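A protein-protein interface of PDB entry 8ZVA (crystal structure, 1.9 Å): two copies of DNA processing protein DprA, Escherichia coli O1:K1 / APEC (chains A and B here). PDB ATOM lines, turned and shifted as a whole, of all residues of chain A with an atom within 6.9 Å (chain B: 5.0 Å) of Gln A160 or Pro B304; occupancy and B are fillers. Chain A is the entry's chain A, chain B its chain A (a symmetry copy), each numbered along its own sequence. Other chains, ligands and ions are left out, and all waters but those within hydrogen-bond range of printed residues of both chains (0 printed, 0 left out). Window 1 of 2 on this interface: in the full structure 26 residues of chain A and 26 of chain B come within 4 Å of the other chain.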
ATOM      1  N   GLN A 155      24.096   1.310 -15.083  1.00  0.00           N
ATOM      2  CA  GLN A 155      24.648   1.553 -16.411  1.00  0.00           C
ATOM      3  C   GLN A 155      24.275   2.941 -16.913  1.00  0.00           C
ATOM      4  O   GLN A 155      25.121   3.662 -17.457  1.00  0.00           O
ATOM      5  CB  GLN A 155      24.157   0.484 -17.388  1.00  0.00           C
ATOM      6  CG  GLN A 155      24.411  -0.943 -16.934  1.00  0.00           C
ATOM      7  CD  GLN A 155      23.626  -1.957 -17.745  1.00  0.00           C
ATOM      8  OE1 GLN A 155      23.907  -2.181 -18.923  1.00  0.00           O
ATOM      9  NE2 GLN A 155      22.635  -2.578 -17.115  1.00  0.00           N
ATOM     10  N   ALA A 156      23.011   3.336 -16.738  1.00  0.00           N
ATOM     11  CA  ALA A 156      22.572   4.642 -17.218  1.00  0.00           C
ATOM     12  C   ALA A 156      23.345   5.766 -16.542  1.00  0.00           C
ATOM     13  O   ALA A 156      23.732   6.744 -17.192  1.00  0.00           O
ATOM     14  CB  ALA A 156      21.071   4.809 -16.981  1.00  0.00           C
ATOM     15  N   VAL A 157      23.575   5.647 -15.233  1.00  0.00           N
ATOM     16  CA  VAL A 157      24.329   6.670 -14.515  1.00  0.00           C
ATOM     17  C   VAL A 157      25.724   6.811 -15.111  1.00  0.00           C
ATOM     18  O   VAL A 157      26.188   7.920 -15.402  1.00  0.00           O
ATOM     19  CB  VAL A 157      24.392   6.331 -13.014  1.00  0.00           C
ATOM     20  CG1 VAL A 157      25.480   7.144 -12.329  1.00  0.00           C
ATOM     21  CG2 VAL A 157      23.041   6.567 -12.356  1.00  0.00           C
ATOM     22  N   ILE A 158      26.416   5.685 -15.290  1.00  0.00           N
ATOM     23  CA  ILE A 158      27.808   5.727 -15.724  1.00  0.00           C
ATOM     24  C   ILE A 158      27.914   6.211 -17.163  1.00  0.00           C
ATOM     25  O   ILE A 158      28.921   6.820 -17.545  1.00  0.00           O
ATOM     26  CB  ILE A 158      28.448   4.339 -15.532  1.00  0.00           C
ATOM     27  CG1 ILE A 158      28.545   4.024 -14.036  1.00  0.00           C
ATOM     28  CG2 ILE A 158      29.817   4.283 -16.187  1.00  0.00           C
ATOM     29  CD1 ILE A 158      28.882   2.584 -13.722  1.00  0.00           C
ATOM     30  N   SER A 159      26.893   5.954 -17.985  1.00  0.00           N
ATOM     31  CA  SER A 159      26.927   6.437 -19.361  1.00  0.00           C
ATOM     32  C   SER A 159      26.960   7.958 -19.416  1.00  0.00           C
ATOM     33  O   SER A 159      27.447   8.535 -20.394  1.00  0.00           O
ATOM     34  CB  SER A 159      25.721   5.903 -20.134  1.00  0.00           C
ATOM     35  OG  SER A 159      24.528   6.545 -19.722  1.00  0.00           O
ATOM     36  N   GLN A 160      26.450   8.625 -18.377  1.00  0.00           N
ATOM     37  CA  GLN A 160      26.459  10.082 -18.355  1.00  0.00           C
ATOM     38  C   GLN A 160      27.872  10.647 -18.318  1.00  0.00           C
ATOM     39  O   GLN A 160      28.076  11.805 -18.702  1.00  0.00           O
ATOM     40  CB  GLN A 160      25.680  10.601 -17.144  1.00  0.00           C
ATOM     41  CG  GLN A 160      24.280  10.033 -16.997  1.00  0.00           C
ATOM     42  CD  GLN A 160      23.406  10.314 -18.201  1.00  0.00           C
ATOM     43  OE1 GLN A 160      23.443  11.406 -18.771  1.00  0.00           O
ATOM     44  NE2 GLN A 160      22.605   9.331 -18.591  1.00  0.00           N
ATOM     45  N   PHE A 161      28.849   9.865 -17.863  1.00  0.00           N
ATOM     46  CA  PHE A 161      30.218  10.331 -17.705  1.00  0.00           C
ATOM     47  C   PHE A 161      31.097   9.988 -18.901  1.00  0.00           C
ATOM     48  O   PHE A 161      32.321  10.124 -18.817  1.00  0.00           O
ATOM     49  CB  PHE A 161      30.820   9.749 -16.425  1.00  0.00           C
ATOM     50  CG  PHE A 161      30.253  10.344 -15.168  1.00  0.00           C
ATOM     51  CD1 PHE A 161      29.030   9.920 -14.673  1.00  0.00           C
ATOM     52  CD2 PHE A 161      30.941  11.333 -14.485  1.00  0.00           C
ATOM     53  CE1 PHE A 161      28.506  10.470 -13.517  1.00  0.00           C
ATOM     54  CE2 PHE A 161      30.422  11.886 -13.329  1.00  0.00           C
ATOM     55  CZ  PHE A 161      29.203  11.454 -12.846  1.00  0.00           C
ATOM     56  N   ILE A 162      30.500   9.553 -20.012  1.00  0.00           N
ATOM     57  CA  ILE A 162      31.281   9.271 -21.206  1.00  0.00           C
ATOM     58  C   ILE A 162      31.920  10.559 -21.706  1.00  0.00           C
ATOM     59  O   ILE A 162      31.277  11.615 -21.771  1.00  0.00           O
ATOM     60  CB  ILE A 162      30.396   8.628 -22.287  1.00  0.00           C
ATOM     61  CG1 ILE A 162      29.954   7.234 -21.837  1.00  0.00           C
ATOM     62  CG2 ILE A 162      31.142   8.551 -23.610  1.00  0.00           C
ATOM     63  CD1 ILE A 162      28.867   6.621 -22.698  1.00  0.00           C
ATOM     64  N   ASP A 163      33.199  10.471 -22.065  1.00  0.00           N
ATOM     65  CA  ASP A 163      33.980  11.603 -22.558  1.00  0.00           C
ATOM     66  C   ASP A 163      34.116  12.713 -21.520  1.00  0.00           C
ATOM     67  O   ASP A 163      34.454  13.851 -21.864  1.00  0.00           O
ATOM     68  CB  ASP A 163      33.388  12.163 -23.857  1.00  0.00           C
ATOM     69  CG  ASP A 163      33.621  11.248 -25.045  1.00  0.00           C
ATOM     70  OD1 ASP A 163      34.316  10.222 -24.880  1.00  0.00           O
ATOM     71  OD2 ASP A 163      33.116  11.556 -26.145  1.00  0.00           O
ATOM     72  N   SER A 164      33.846  12.411 -20.256  1.00  0.00           N
ATOM     73  CA  SER A 164      34.265  13.266 -19.157  1.00  0.00           C
ATOM     74  C   SER A 164      35.694  12.898 -18.764  1.00  0.00           C
ATOM     75  O   SER A 164      36.270  11.927 -19.261  1.00  0.00           O
ATOM     76  CB  SER A 164      33.318  13.123 -17.966  1.00  0.00           C
ATOM     77  OG  SER A 164      33.484  11.873 -17.319  1.00  0.00           O
ATOM     78  N   PHE A 187      31.590   1.276 -21.717  1.00  0.00           N
ATOM     79  CA  PHE A 187      31.656   2.639 -22.228  1.00  0.00           C
ATOM     80  C   PHE A 187      33.076   3.189 -22.259  1.00  0.00           C
ATOM     81  O   PHE A 187      33.262   4.377 -22.545  1.00  0.00           O
ATOM     82  CB  PHE A 187      30.764   3.557 -21.386  1.00  0.00           C
ATOM     83  CG  PHE A 187      29.354   3.058 -21.230  1.00  0.00           C
ATOM     84  CD1 PHE A 187      28.681   2.491 -22.300  1.00  0.00           C
ATOM     85  CD2 PHE A 187      28.702   3.158 -20.013  1.00  0.00           C
ATOM     86  CE1 PHE A 187      27.385   2.031 -22.158  1.00  0.00           C
ATOM     87  CE2 PHE A 187      27.406   2.700 -19.864  1.00  0.00           C
ATOM     88  CZ  PHE A 187      26.748   2.136 -20.938  1.00  0.00           C
ATOM     89  N   ILE A 189      35.176   3.864 -19.895  1.00  0.00           N
ATOM     90  CA  ILE A 189      35.540   4.744 -18.795  1.00  0.00           C
ATOM     91  C   ILE A 189      36.486   3.967 -17.879  1.00  0.00           C
ATOM     92  O   ILE A 189      36.118   2.869 -17.431  1.00  0.00           O
ATOM     93  CB  ILE A 189      34.310   5.227 -18.020  1.00  0.00           C
ATOM     94  CG1 ILE A 189      33.375   6.018 -18.939  1.00  0.00           C
ATOM     95  CG2 ILE A 189      34.723   6.079 -16.831  1.00  0.00           C
ATOM     96  CD1 ILE A 189      31.996   6.260 -18.351  1.00  0.00           C
ATOM     97  N   MET A 301      19.381  12.870  -9.163  1.00  0.00           N
ATOM     98  CA  MET A 301      19.821  12.857 -10.555  1.00  0.00           C
ATOM     99  C   MET A 301      18.786  12.093 -11.368  1.00  0.00           C
ATOM    100  O   MET A 301      18.717  10.862 -11.293  1.00  0.00           O
ATOM    101  CB  MET A 301      21.199  12.227 -10.714  1.00  0.00           C
ATOM    102  CG  MET A 301      21.602  12.143 -12.198  1.00  0.00           C
ATOM    103  SD  MET A 301      23.318  11.666 -12.453  1.00  0.00           S
ATOM    104  CE  MET A 301      23.294  10.020 -11.755  1.00  0.00           C
ATOM    105  N   ASN A 302      17.994  12.820 -12.149  1.00  0.00           N
ATOM    106  CA  ASN A 302      16.959  12.201 -12.963  1.00  0.00           C
ATOM    107  C   ASN A 302      17.574  11.300 -14.022  1.00  0.00           C
ATOM    108  O   ASN A 302      18.532  11.680 -14.699  1.00  0.00           O
ATOM    109  CB  ASN A 302      16.112  13.282 -13.630  1.00  0.00           C
ATOM    110  CG  ASN A 302      15.331  14.112 -12.625  1.00  0.00           C
ATOM    111  OD1 ASN A 302      14.718  13.578 -11.702  1.00  0.00           O
ATOM    112  ND2 ASN A 302      15.339  15.426 -12.813  1.00  0.00           N
ATOM    113  N   ILE A 303      17.022  10.100 -14.155  1.00  0.00           N
ATOM    114  CA  ILE A 303      17.403   9.182 -15.224  1.00  0.00           C
ATOM    115  C   ILE A 303      16.153   8.863 -16.036  1.00  0.00           C
ATOM    116  O   ILE A 303      15.247   8.181 -15.534  1.00  0.00           O
ATOM    117  CB  ILE A 303      18.052   7.907 -14.664  1.00  0.00           C
ATOM    118  CG1 ILE A 303      19.267   8.263 -13.799  1.00  0.00           C
ATOM    119  CG2 ILE A 303      18.463   6.969 -15.796  1.00  0.00           C
ATOM    120  CD1 ILE A 303      20.382   8.963 -14.565  1.00  0.00           C
ATOM    121  N   PRO A 304      16.058   9.321 -17.294  1.00  0.00           N
ATOM    122  CA  PRO A 304      17.099  10.114 -17.965  1.00  0.00           C
ATOM    123  C   PRO A 304      17.186  11.555 -17.456  1.00  0.00           C
ATOM    124  O   PRO A 304      16.220  12.074 -16.893  1.00  0.00           O
ATOM    125  CB  PRO A 304      16.678  10.088 -19.445  1.00  0.00           C
ATOM    126  CG  PRO A 304      15.566   9.058 -19.545  1.00  0.00           C
ATOM    127  CD  PRO A 304      14.927   9.026 -18.190  1.00  0.00           C
ATOM    128  N   LEU A 305      18.354  12.180 -17.631  1.00  0.00           N
ATOM    129  CA  LEU A 305      18.459  13.617 -17.408  1.00  0.00           C
ATOM    130  C   LEU A 305      17.730  14.385 -18.501  1.00  0.00           C
ATOM    131  O   LEU A 305      17.219  15.484 -18.258  1.00  0.00           O
ATOM    132  CB  LEU A 305      19.927  14.039 -17.364  1.00  0.00           C
ATOM    133  CG  LEU A 305      20.727  13.654 -16.121  1.00  0.00           C
ATOM    134  CD1 LEU A 305      22.216  13.860 -16.371  1.00  0.00           C
ATOM    135  CD2 LEU A 305      20.267  14.459 -14.917  1.00  0.00           C
ATOM    136  N   SER A 306      17.675  13.815 -19.702  1.00  0.00           N
ATOM    137  CA  SER A 306      16.932  14.390 -20.808  1.00  0.00           C
ATOM    138  C   SER A 306      15.443  14.447 -20.491  1.00  0.00           C
ATOM    139  O   SER A 306      14.928  13.711 -19.648  1.00  0.00           O
ATOM    140  CB  SER A 306      17.152  13.555 -22.068  1.00  0.00           C
ATOM    141  OG  SER A 306      16.736  12.215 -21.846  1.00  0.00           O
ATOM    142  N   ARG B 281      27.528   8.229 -27.235  1.00  0.00           N
ATOM    143  CA  ARG B 281      28.346   9.434 -27.230  1.00  0.00           C
ATOM    144  C   ARG B 281      29.801   9.097 -27.528  1.00  0.00           C
ATOM    145  O   ARG B 281      30.354   8.138 -26.983  1.00  0.00           O
ATOM    146  CB  ARG B 281      28.235  10.133 -25.874  1.00  0.00           C
ATOM    147  CG  ARG B 281      29.010  11.439 -25.774  1.00  0.00           C
ATOM    148  CD  ARG B 281      29.091  11.927 -24.332  1.00  0.00           C
ATOM    149  NE  ARG B 281      27.778  12.279 -23.798  1.00  0.00           N
ATOM    150  CZ  ARG B 281      27.516  12.463 -22.507  1.00  0.00           C
ATOM    151  NH1 ARG B 281      28.478  12.325 -21.605  1.00  0.00           N
ATOM    152  NH2 ARG B 281      26.288  12.781 -22.118  1.00  0.00           N
ATOM    153  N   ASN B 302      21.492  10.689 -30.235  1.00  0.00           N
ATOM    154  CA  ASN B 302      22.609  10.532 -29.314  1.00  0.00           C
ATOM    155  C   ASN B 302      22.158   9.842 -28.036  1.00  0.00           C
ATOM    156  O   ASN B 302      21.124  10.189 -27.459  1.00  0.00           O
ATOM    157  CB  ASN B 302      23.202  11.899 -28.984  1.00  0.00           C
ATOM    158  CG  ASN B 302      23.827  12.570 -30.195  1.00  0.00           C
ATOM    159  OD1 ASN B 302      24.561  11.943 -30.959  1.00  0.00           O
ATOM    160  ND2 ASN B 302      23.550  13.856 -30.366  1.00  0.00           N
ATOM    161  N   ILE B 303      22.936   8.859 -27.600  1.00  0.00           N
ATOM    162  CA  ILE B 303      22.719   8.204 -26.315  1.00  0.00           C
ATOM    163  C   ILE B 303      23.984   8.372 -25.482  1.00  0.00           C
ATOM    164  O   ILE B 303      25.023   7.777 -25.808  1.00  0.00           O
ATOM    165  CB  ILE B 303      22.355   6.722 -26.496  1.00  0.00           C
ATOM    166  CG1 ILE B 303      21.117   6.581 -27.389  1.00  0.00           C
ATOM    167  CG2 ILE B 303      22.109   6.059 -25.143  1.00  0.00           C
ATOM    168  CD1 ILE B 303      19.863   7.221 -26.810  1.00  0.00           C
ATOM    169  N   PRO B 304      23.950   9.159 -24.395  1.00  0.00           N
ATOM    170  CA  PRO B 304      22.752   9.877 -23.934  1.00  0.00           C
ATOM    171  C   PRO B 304      22.392  11.081 -24.807  1.00  0.00           C
ATOM    172  O   PRO B 304      23.248  11.614 -25.515  1.00  0.00           O
ATOM    173  CB  PRO B 304      23.129  10.333 -22.514  1.00  0.00           C
ATOM    174  CG  PRO B 304      24.422   9.613 -22.171  1.00  0.00           C
ATOM    175  CD  PRO B 304      25.091   9.348 -23.486  1.00  0.00           C
ATOM    176  N   LEU B 305      21.118  11.482 -24.773  1.00  0.00           N
ATOM    177  CA  LEU B 305      20.731  12.755 -25.370  1.00  0.00           C
ATOM    178  C   LEU B 305      21.261  13.918 -24.544  1.00  0.00           C
ATOM    179  O   LEU B 305      21.547  14.991 -25.086  1.00  0.00           O
ATOM    180  CB  LEU B 305      19.210  12.846 -25.485  1.00  0.00           C
ATOM    181  CG  LEU B 305      18.539  11.989 -26.557  1.00  0.00           C
ATOM    182  CD1 LEU B 305      17.032  11.950 -26.330  1.00  0.00           C
ATOM    183  CD2 LEU B 305      18.861  12.517 -27.944  1.00  0.00           C
ATOM    184  N   SER B 306      21.396  13.713 -23.236  1.00  0.00           N
ATOM    185  CA  SER B 306      21.977  14.700 -22.344  1.00  0.00           C
ATOM    186  C   SER B 306      23.432  14.969 -22.706  1.00  0.00           C
ATOM    187  O   SER B 306      24.108  14.153 -23.335  1.00  0.00           O
ATOM    188  CB  SER B 306      21.894  14.207 -20.901  1.00  0.00           C
ATOM    189  OG  SER B 306      22.577  12.968 -20.769  1.00  0.00           O
ATOM    190  N   PHE B 308      27.228  16.131 -20.833  1.00  0.00           N
ATOM    191  CA  PHE B 308      27.877  16.097 -19.529  1.00  0.00           C
ATOM    192  C   PHE B 308      27.698  17.411 -18.781  1.00  0.00           C
ATOM    193  O   PHE B 308      27.790  17.428 -17.548  1.00  0.00           O
ATOM    194  CB  PHE B 308      29.366  15.788 -19.675  1.00  0.00           C
ATOM    195  CG  PHE B 308      30.079  15.614 -18.362  1.00  0.00           C
ATOM    196  CD1 PHE B 308      29.688  14.628 -17.471  1.00  0.00           C
ATOM    197  CD2 PHE B 308      31.138  16.438 -18.020  1.00  0.00           C
ATOM    198  CE1 PHE B 308      30.340  14.467 -16.262  1.00  0.00           C
ATOM    199  CE2 PHE B 308      31.795  16.280 -16.813  1.00  0.00           C
ATOM    200  CZ  PHE B 308      31.395  15.295 -15.934  1.00  0.00           C
ATOM    201  N   VAL B 311      25.284  17.108 -16.143  1.00  0.00           N
ATOM    202  CA  VAL B 311      25.781  16.444 -14.944  1.00  0.00           C
ATOM    203  C   VAL B 311      26.566  17.425 -14.085  1.00  0.00           C
ATOM    204  O   VAL B 311      26.467  17.411 -12.852  1.00  0.00           O
ATOM    205  CB  VAL B 311      26.638  15.222 -15.327  1.00  0.00           C
ATOM    206  CG1 VAL B 311      27.100  14.483 -14.077  1.00  0.00           C
ATOM    207  CG2 VAL B 311      25.861  14.292 -16.249  1.00  0.00           C
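O of Gln A160 lies within hydrogen-bond range of NH1 of Arg B281, 3.0 Å away.
The side-chain amide oxygen of Gln A160 lies within hydrogen-bond range of the side-chain hydroxyl of Ser B306, at 2.7 Å.
The backbone carbonyl oxygen (O) of Ile A162 sits at hydrogen-bond distance from the guanidinium group (NH1) of Arg B281.
O of Ala A156 is in hydrogen-bond range of OG of Ser A159.
O of Ala A156 lies within hydrogen-bond range of NE2 of Gln A160, 3.1 Å away.
The backbone carbonyl oxygen of Phe A161 sits at hydrogen-bond distance from the side-chain hydroxyl of Ser A164 (2.6 Å).
The backbone NH (N) of Arg B281 lies within hydrogen-bond range of the backbone carbonyl oxygen (O) of Ile B303 (2.9 Å).
NH2 of Arg B281 lies within hydrogen-bond range of O of Ser B306 (2.8 Å).
Among the printed residues, merely in contact across the chains: Gln A160 with Phe B308, Ser A164 with Phe B308, Phe A161 with Phe B308, Ser A159 with Pro B304, Leu A305 with Val B311, Gln A160 with Val B311, Phe A161 with Val B311 and Gln A160 with Pro B304.
Of the printed residues of chain B, Ser A159 touches Pro B304.
Of chain B, only Arg B281 (3.0 Å), Pro B304 (3.9 Å), Ser B306 (2.7 Å), Phe B308 (3.5 Å) and Val B311 (3.8 Å) come within 4 Å of Gln A160.
Of the printed residues of chain B, Ser A164 touches Phe B308 (3.5 Å).
Phe A187 touches none of the printed residues of chain B.
Of chain A, only Ser A159 and Gln A160 come within 4 Å of Pro B304.
Of the printed residues of chain A, Ser B306 touches Gln A160.
The nearest printed residue of chain B that does not touch Gln A160 is Leu B305 (6.4 Å).
The nearest residue of chain A that does not touch Pro B304 is Ile A162 (4.7 Å).
Printed residues of chain B that touch a printed residue of chain A: Arg B281, Pro B304, Ser B306, Phe B308 and Val B311.
Printed residues of chain A that touch a printed residue of chain B: Ser A159, Gln A160, Phe A161, Ile A162, Ser A164 and Leu A305.
Among the printed residues, no Asp or Glu carboxylate lies within 4 Å of a Lys or Arg side-chain nitrogen of the other chain.
Positions printed for both chains: 302, 303, 304, 305 and 306.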
